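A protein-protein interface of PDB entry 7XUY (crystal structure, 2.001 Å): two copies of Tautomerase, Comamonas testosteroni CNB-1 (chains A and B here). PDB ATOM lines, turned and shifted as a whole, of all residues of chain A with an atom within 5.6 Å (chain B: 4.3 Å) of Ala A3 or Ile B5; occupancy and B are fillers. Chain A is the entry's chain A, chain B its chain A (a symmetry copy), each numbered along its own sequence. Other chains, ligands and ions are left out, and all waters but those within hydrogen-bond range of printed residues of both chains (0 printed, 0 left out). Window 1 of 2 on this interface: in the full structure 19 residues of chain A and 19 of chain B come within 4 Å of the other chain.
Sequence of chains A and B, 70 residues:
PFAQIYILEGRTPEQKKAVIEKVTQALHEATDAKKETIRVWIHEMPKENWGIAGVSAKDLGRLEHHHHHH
Printed residues of chain A that touch a printed residue of chain B: Pro A1, Phe A2, Ala A3, Gln A4, Ile A5 and Leu A27. Hydrophobic or aromatic side chains of chain A that line the printed part of chain B: Pro A1, Ala A3, Ile A5 and Leu A27. Of the 10 printed residues of chain B, 5 touch a printed residue of chain A. Printed residues of chain B that touch a printed residue of chain A: Ala B3, Gln B4, Ile B5, Tyr B6 and Ile B7. Hydrophobic or aromatic side chains of chain B within 4 Å of the printed part of chain A: Ala B3, Ile B5, Tyr B6 and Ile B7. Among the printed residues, no Asp or Glu carboxylate lies within 4 Å of a Lys or Arg side-chain nitrogen of the other chain.
Among the printed residues, merely in contact across the chains: Pro A1 with Tyr B6, Pro A1 with Ile B7, Phe A2 with Gln B4, Phe A2 with Ile B5, Ala A3 with Gln B4, Ala A3 with Ile B5, Gln A4 with Ala B3, Ile A5 with Ala B3 and Leu A27 with Ile B5.
N of Tyr B6 is in hydrogen-bond range of O of Phe A2 (2.8 Å). The backbone NH of Gln A4 lies within hydrogen-bond range of the backbone carbonyl oxygen of Gln B4. The side-chain amide oxygen of Gln A4 is in hydrogen-bond range of the side-chain hydroxyl of Tyr B6.
Ala A3 touches Gln B4, and with the chains exchanged Gln A4 touches Ala B3. Ala A3 touches Ile B5, and with the chains exchanged Ile A5 touches Ala B3. Gln A4 touches its own counterpart, Gln B4. Positions printed for both chains: 3, 4, 5, 40 and 41. Of the 12 pairs that touch across the chains among the printed residues, 5 have their exchanged pair printed and touching as well.
Ala A3 touches just these residues of chain B: Gln B4 and Ile B5. Of the printed residues of chain B, Leu A27 touches Ile B5 (3.9 Å). Of the printed residues of chain A, Gln B4 touches Phe A2 (3.9 Å), Ala A3 (3.5 Å) and Gln A4 (2.8 Å). Of chain A, only Phe A2, Ala A3 and Leu A27 come within 4 Å of Ile B5. Printed residues of chain A within 4 Å of Tyr B6: Pro A1, Phe A2 and Gln A4. The nearest printed residue of chain B that does not touch Ala A3 is Tyr B6 (5.0 Å). The nearest residue of chain A that does not touch Ile B5 is Gln A4 (4.9 Å).
The backbone carbonyl oxygen of Ala A3 sits at hydrogen-bond distance from the backbone NH of Trp A41 (3.0 Å). The indole nitrogen (NE1) of Trp A41 lies close to the side-chain amide nitrogen (NE2) of Gln A4, 3.4 Å away. OE1 of Gln B4 lies close to OH of Tyr B6, 3.3 Å away. NE2 of Gln B4 lies close to NE1 of Trp B41 (3.4 Å). The backbone carbonyl oxygen of Trp B41 lies within hydrogen-bond range of the backbone NH of Ile B5. The backbone NH (N) of Ile B7 sits at hydrogen-bond distance from the backbone carbonyl oxygen (O) of His B43.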
ATOM      1  N   PRO A   1      17.740 -11.719  11.430  1.00  0.00           N
ATOM      2  CA  PRO A   1      16.469 -11.084  11.810  1.00  0.00           C
ATOM      3  C   PRO A   1      16.612  -9.570  11.922  1.00  0.00           C
ATOM      4  O   PRO A   1      17.642  -9.066  12.384  1.00  0.00           O
ATOM      5  CB  PRO A   1      16.141 -11.718  13.163  1.00  0.00           C
ATOM      6  CG  PRO A   1      17.400 -12.364  13.617  1.00  0.00           C
ATOM      7  CD  PRO A   1      18.140 -12.757  12.384  1.00  0.00           C
ATOM      8  N   PHE A   2      15.597  -8.852  11.464  1.00  0.00           N
ATOM      9  CA  PHE A   2      15.630  -7.404  11.364  1.00  0.00           C
ATOM     10  C   PHE A   2      14.507  -6.842  12.207  1.00  0.00           C
ATOM     11  O   PHE A   2      13.434  -7.436  12.258  1.00  0.00           O
ATOM     12  CB  PHE A   2      15.410  -6.942   9.941  1.00  0.00           C
ATOM     13  CG  PHE A   2      16.458  -7.375   8.998  1.00  0.00           C
ATOM     14  CD1 PHE A   2      17.686  -7.842   9.461  1.00  0.00           C
ATOM     15  CD2 PHE A   2      16.236  -7.297   7.642  1.00  0.00           C
ATOM     16  CE1 PHE A   2      18.661  -8.245   8.578  1.00  0.00           C
ATOM     17  CE2 PHE A   2      17.226  -7.705   6.747  1.00  0.00           C
ATOM     18  CZ  PHE A   2      18.423  -8.172   7.220  1.00  0.00           C
ATOM     19  N   ALA A   3      14.737  -5.694  12.841  1.00  0.00           N
ATOM     20  CA  ALA A   3      13.662  -5.001  13.549  1.00  0.00           C
ATOM     21  C   ALA A   3      13.587  -3.566  13.054  1.00  0.00           C
ATOM     22  O   ALA A   3      14.590  -2.844  13.066  1.00  0.00           O
ATOM     23  CB  ALA A   3      13.859  -5.022  15.067  1.00  0.00           C
ATOM     24  N   GLN A   4      12.411  -3.168  12.623  1.00  0.00           N
ATOM     25  CA  GLN A   4      12.116  -1.794  12.238  1.00  0.00           C
ATOM     26  C   GLN A   4      11.316  -1.173  13.376  1.00  0.00           C
ATOM     27  O   GLN A   4      10.200  -1.613  13.657  1.00  0.00           O
ATOM     28  CB  GLN A   4      11.323  -1.784  10.931  1.00  0.00           C
ATOM     29  CG  GLN A   4      10.943  -0.411  10.382  1.00  0.00           C
ATOM     30  CD  GLN A   4      10.598  -0.491   8.876  1.00  0.00           C
ATOM     31  OE1 GLN A   4      10.170  -1.543   8.386  1.00  0.00           O
ATOM     32  NE2 GLN A   4      10.836   0.574   8.155  1.00  0.00           N
ATOM     33  N   ILE A   5      11.886  -0.183  14.053  1.00  0.00           N
ATOM     34  CA  ILE A   5      11.287   0.379  15.262  1.00  0.00           C
ATOM     35  C   ILE A   5      10.680   1.726  14.920  1.00  0.00           C
ATOM     36  O   ILE A   5      11.301   2.531  14.219  1.00  0.00           O
ATOM     37  CB  ILE A   5      12.322   0.541  16.390  1.00  0.00           C
ATOM     38  CG1 ILE A   5      13.146  -0.742  16.551  1.00  0.00           C
ATOM     39  CG2 ILE A   5      11.616   0.950  17.705  1.00  0.00           C
ATOM     40  CD1 ILE A   5      12.290  -1.973  16.714  1.00  0.00           C
ATOM     41  N   VAL A  23      16.926  -4.481  21.823  1.00  0.00           N
ATOM     42  CA  VAL A  23      16.177  -5.196  20.794  1.00  0.00           C
ATOM     43  C   VAL A  23      17.070  -6.220  20.106  1.00  0.00           C
ATOM     44  O   VAL A  23      16.640  -7.346  19.831  1.00  0.00           O
ATOM     45  CB  VAL A  23      15.554  -4.209  19.791  1.00  0.00           C
ATOM     46  CG1 VAL A  23      14.933  -4.956  18.608  1.00  0.00           C
ATOM     47  CG2 VAL A  23      14.526  -3.353  20.490  1.00  0.00           C
ATOM     48  N   LEU A  27      16.324 -10.234  20.102  1.00  0.00           N
ATOM     49  CA  LEU A  27      16.225 -11.094  18.927  1.00  0.00           C
ATOM     50  C   LEU A  27      17.251 -12.221  18.984  1.00  0.00           C
ATOM     51  O   LEU A  27      16.957 -13.357  18.591  1.00  0.00           O
ATOM     52  CB  LEU A  27      16.400 -10.269  17.653  1.00  0.00           C
ATOM     53  CG  LEU A  27      15.279  -9.306  17.223  1.00  0.00           C
ATOM     54  CD1 LEU A  27      15.684  -8.597  15.940  1.00  0.00           C
ATOM     55  CD2 LEU A  27      13.933 -10.023  17.031  1.00  0.00           C
ATOM     56  N   ARG A  39      19.882  -6.756  12.553  1.00  0.00           N
ATOM     57  CA  ARG A  39      19.852  -5.349  12.202  1.00  0.00           C
ATOM     58  C   ARG A  39      18.619  -4.714  12.819  1.00  0.00           C
ATOM     59  O   ARG A  39      17.523  -5.285  12.768  1.00  0.00           O
ATOM     60  CB  ARG A  39      19.805  -5.156  10.682  1.00  0.00           C
ATOM     61  CG  ARG A  39      20.910  -5.841   9.915  1.00  0.00           C
ATOM     62  CD  ARG A  39      22.142  -4.978   9.905  1.00  0.00           C
ATOM     63  NE  ARG A  39      23.219  -5.573   9.120  1.00  0.00           N
ATOM     64  CZ  ARG A  39      23.898  -6.663   9.472  1.00  0.00           C
ATOM     65  NH1 ARG A  39      23.595  -7.306  10.594  1.00  0.00           N
ATOM     66  NH2 ARG A  39      24.876  -7.130   8.698  1.00  0.00           N
ATOM     67  N   VAL A  40      18.793  -3.526  13.388  1.00  0.00           N
ATOM     68  CA  VAL A  40      17.707  -2.787  14.017  1.00  0.00           C
ATOM     69  C   VAL A  40      17.848  -1.332  13.601  1.00  0.00           C
ATOM     70  O   VAL A  40      18.927  -0.745  13.754  1.00  0.00           O
ATOM     71  CB  VAL A  40      17.755  -2.885  15.554  1.00  0.00           C
ATOM     72  CG1 VAL A  40      16.616  -2.090  16.154  1.00  0.00           C
ATOM     73  CG2 VAL A  40      17.738  -4.339  16.026  1.00  0.00           C
ATOM     74  N   TRP A  41      16.785  -0.747  13.079  1.00  0.00           N
ATOM     75  CA  TRP A  41      16.837   0.665  12.736  1.00  0.00           C
ATOM     76  C   TRP A  41      15.584   1.352  13.271  1.00  0.00           C
ATOM     77  O   TRP A  41      14.565   0.709  13.535  1.00  0.00           O
ATOM     78  CB  TRP A  41      17.033   0.871  11.219  1.00  0.00           C
ATOM     79  CG  TRP A  41      15.936   0.405  10.310  1.00  0.00           C
ATOM     80  CD1 TRP A  41      14.931   1.170   9.772  1.00  0.00           C
ATOM     81  CD2 TRP A  41      15.759  -0.918   9.779  1.00  0.00           C
ATOM     82  NE1 TRP A  41      14.142   0.395   8.945  1.00  0.00           N
ATOM     83  CE2 TRP A  41      14.627  -0.888   8.941  1.00  0.00           C
ATOM     84  CE3 TRP A  41      16.450  -2.128   9.939  1.00  0.00           C
ATOM     85  CZ2 TRP A  41      14.157  -2.025   8.272  1.00  0.00           C
ATOM     86  CZ3 TRP A  41      15.981  -3.249   9.270  1.00  0.00           C
ATOM     87  CH2 TRP A  41      14.845  -3.183   8.447  1.00  0.00           C
ATOM     88  N   ALA B   3       7.395  -2.268  17.010  1.00  0.00           N
ATOM     89  CA  ALA B   3       8.491  -2.978  16.351  1.00  0.00           C
ATOM     90  C   ALA B   3       7.919  -3.867  15.259  1.00  0.00           C
ATOM     91  O   ALA B   3       7.025  -4.681  15.515  1.00  0.00           O
ATOM     92  CB  ALA B   3       9.311  -3.818  17.333  1.00  0.00           C
ATOM     93  N   GLN B   4       8.431  -3.704  14.060  1.00  0.00           N
ATOM     94  CA  GLN B   4       8.105  -4.554  12.921  1.00  0.00           C
ATOM     95  C   GLN B   4       9.285  -5.495  12.715  1.00  0.00           C
ATOM     96  O   GLN B   4      10.387  -5.044  12.400  1.00  0.00           O
ATOM     97  CB  GLN B   4       7.863  -3.688  11.685  1.00  0.00           C
ATOM     98  CG  GLN B   4       7.496  -4.431  10.402  1.00  0.00           C
ATOM     99  CD  GLN B   4       6.815  -3.483   9.387  1.00  0.00           C
ATOM    100  OE1 GLN B   4       7.051  -2.269   9.407  1.00  0.00           O
ATOM    101  NE2 GLN B   4       5.949  -4.017   8.565  1.00  0.00           N
ATOM    102  N   ILE B   5       9.076  -6.790  12.924  1.00  0.00           N
ATOM    103  CA  ILE B   5      10.164  -7.765  12.916  1.00  0.00           C
ATOM    104  C   ILE B   5      10.103  -8.548  11.619  1.00  0.00           C
ATOM    105  O   ILE B   5       9.022  -8.964  11.191  1.00  0.00           O
ATOM    106  CB  ILE B   5      10.076  -8.728  14.115  1.00  0.00           C
ATOM    107  CG1 ILE B   5       9.848  -7.948  15.415  1.00  0.00           C
ATOM    108  CG2 ILE B   5      11.345  -9.612  14.180  1.00  0.00           C
ATOM    109  CD1 ILE B   5      10.855  -6.845  15.622  1.00  0.00           C
ATOM    110  N   TYR B   6      11.259  -8.776  11.013  1.00  0.00           N
ATOM    111  CA  TYR B   6      11.369  -9.614   9.825  1.00  0.00           C
ATOM    112  C   TYR B   6      12.259 -10.801  10.154  1.00  0.00           C
ATOM    113  O   TYR B   6      13.435 -10.618  10.495  1.00  0.00           O
ATOM    114  CB  TYR B   6      11.941  -8.829   8.642  1.00  0.00           C
ATOM    115  CG  TYR B   6      11.184  -7.554   8.348  1.00  0.00           C
ATOM    116  CD1 TYR B   6      10.092  -7.559   7.499  1.00  0.00           C
ATOM    117  CD2 TYR B   6      11.565  -6.342   8.925  1.00  0.00           C
ATOM    118  CE1 TYR B   6       9.376  -6.397   7.249  1.00  0.00           C
ATOM    119  CE2 TYR B   6      10.870  -5.169   8.647  1.00  0.00           C
ATOM    120  CZ  TYR B   6       9.774  -5.210   7.822  1.00  0.00           C
ATOM    121  OH  TYR B   6       9.085  -4.042   7.553  1.00  0.00           O
ATOM    122  N   ILE B   7      11.701 -12.014  10.062  1.00  0.00           N
ATOM    123  CA  ILE B   7      12.467 -13.245  10.255  1.00  0.00           C
ATOM    124  C   ILE B   7      12.205 -14.165   9.072  1.00  0.00           C
ATOM    125  O   ILE B   7      11.191 -14.052   8.374  1.00  0.00           O
ATOM    126  CB  ILE B   7      12.114 -13.992  11.568  1.00  0.00           C
ATOM    127  CG1 ILE B   7      10.623 -14.358  11.593  1.00  0.00           C
ATOM    128  CG2 ILE B   7      12.475 -13.161  12.808  1.00  0.00           C
ATOM    129  CD1 ILE B   7      10.203 -15.228  12.791  1.00  0.00           C
ATOM    130  N   VAL B  19      10.071 -13.748  20.661  1.00  0.00           N
ATOM    131  CA  VAL B  19      10.323 -12.485  19.970  1.00  0.00           C
ATOM    132  C   VAL B  19       9.373 -11.416  20.491  1.00  0.00           C
ATOM    133  O   VAL B  19       9.791 -10.319  20.880  1.00  0.00           O
ATOM    134  CB  VAL B  19      10.195 -12.646  18.441  1.00  0.00           C
ATOM    135  CG1 VAL B  19      10.149 -11.261  17.760  1.00  0.00           C
ATOM    136  CG2 VAL B  19      11.345 -13.464  17.863  1.00  0.00           C
ATOM    137  N   VAL B  40       4.261  -5.215  18.725  1.00  0.00           N
ATOM    138  CA  VAL B  40       5.303  -5.917  17.991  1.00  0.00           C
ATOM    139  C   VAL B  40       4.618  -6.912  17.069  1.00  0.00           C
ATOM    140  O   VAL B  40       3.786  -7.708  17.524  1.00  0.00           O
ATOM    141  CB  VAL B  40       6.265  -6.672  18.930  1.00  0.00           C
ATOM    142  CG1 VAL B  40       7.317  -7.393  18.116  1.00  0.00           C
ATOM    143  CG2 VAL B  40       6.894  -5.735  19.962  1.00  0.00           C
ATOM    144  N   TRP B  41       4.947  -6.877  15.790  1.00  0.00           N
ATOM    145  CA  TRP B  41       4.384  -7.856  14.876  1.00  0.00           C
ATOM    146  C   TRP B  41       5.502  -8.430  14.011  1.00  0.00           C
ATOM    147  O   TRP B  41       6.566  -7.825  13.856  1.00  0.00           O
ATOM    148  CB  TRP B  41       3.231  -7.254  14.044  1.00  0.00           C
ATOM    149  CG  TRP B  41       3.569  -6.148  13.091  1.00  0.00           C
ATOM    150  CD1 TRP B  41       3.807  -6.263  11.744  1.00  0.00           C
ATOM    151  CD2 TRP B  41       3.653  -4.745  13.393  1.00  0.00           C
ATOM    152  NE1 TRP B  41       4.037  -5.016  11.198  1.00  0.00           N
ATOM    153  CE2 TRP B  41       3.954  -4.074  12.191  1.00  0.00           C
ATOM    154  CE3 TRP B  41       3.506  -3.995  14.569  1.00  0.00           C
ATOM    155  CZ2 TRP B  41       4.127  -2.685  12.129  1.00  0.00           C
ATOM    156  CZ3 TRP B  41       3.675  -2.620  14.498  1.00  0.00           C
ATOM    157  CH2 TRP B  41       3.980  -1.985  13.284  1.00  0.00           C
ATOM    158  N   ILE B  42       5.265  -9.619  13.461  1.00  0.00           N
ATOM    159  CA  ILE B  42       6.332 -10.424  12.865  1.00  0.00           C
ATOM    160  C   ILE B  42       5.923 -10.824  11.457  1.00  0.00           C
ATOM    161  O   ILE B  42       4.886 -11.474  11.274  1.00  0.00           O
ATOM    162  CB  ILE B  42       6.637 -11.685  13.702  1.00  0.00           C
ATOM    163  CG1 ILE B  42       7.012 -11.313  15.145  1.00  0.00           C
ATOM    164  CG2 ILE B  42       7.736 -12.502  13.048  1.00  0.00           C
ATOM    165  CD1 ILE B  42       7.115 -12.540  16.107  1.00  0.00           C
ATOM    166  N   HIS B  43       6.748 -10.454  10.471  1.00  0.00           N
ATOM    167  CA  HIS B  43       6.656 -10.967   9.112  1.00  0.00           C
ATOM    168  C   HIS B  43       7.603 -12.149   8.966  1.00  0.00           C
ATOM    169  O   HIS B  43       8.817 -12.006   9.194  1.00  0.00           O
ATOM    170  CB  HIS B  43       7.034  -9.891   8.090  1.00  0.00           C
ATOM    171  CG  HIS B  43       6.204  -8.648   8.169  1.00  0.00           C
ATOM    172  ND1 HIS B  43       5.001  -8.523   7.518  1.00  0.00           N
ATOM    173  CD2 HIS B  43       6.406  -7.477   8.820  1.00  0.00           C
ATOM    174  CE1 HIS B  43       4.487  -7.333   7.768  1.00  0.00           C
ATOM    175  NE2 HIS B  43       5.329  -6.672   8.547  1.00  0.00           N
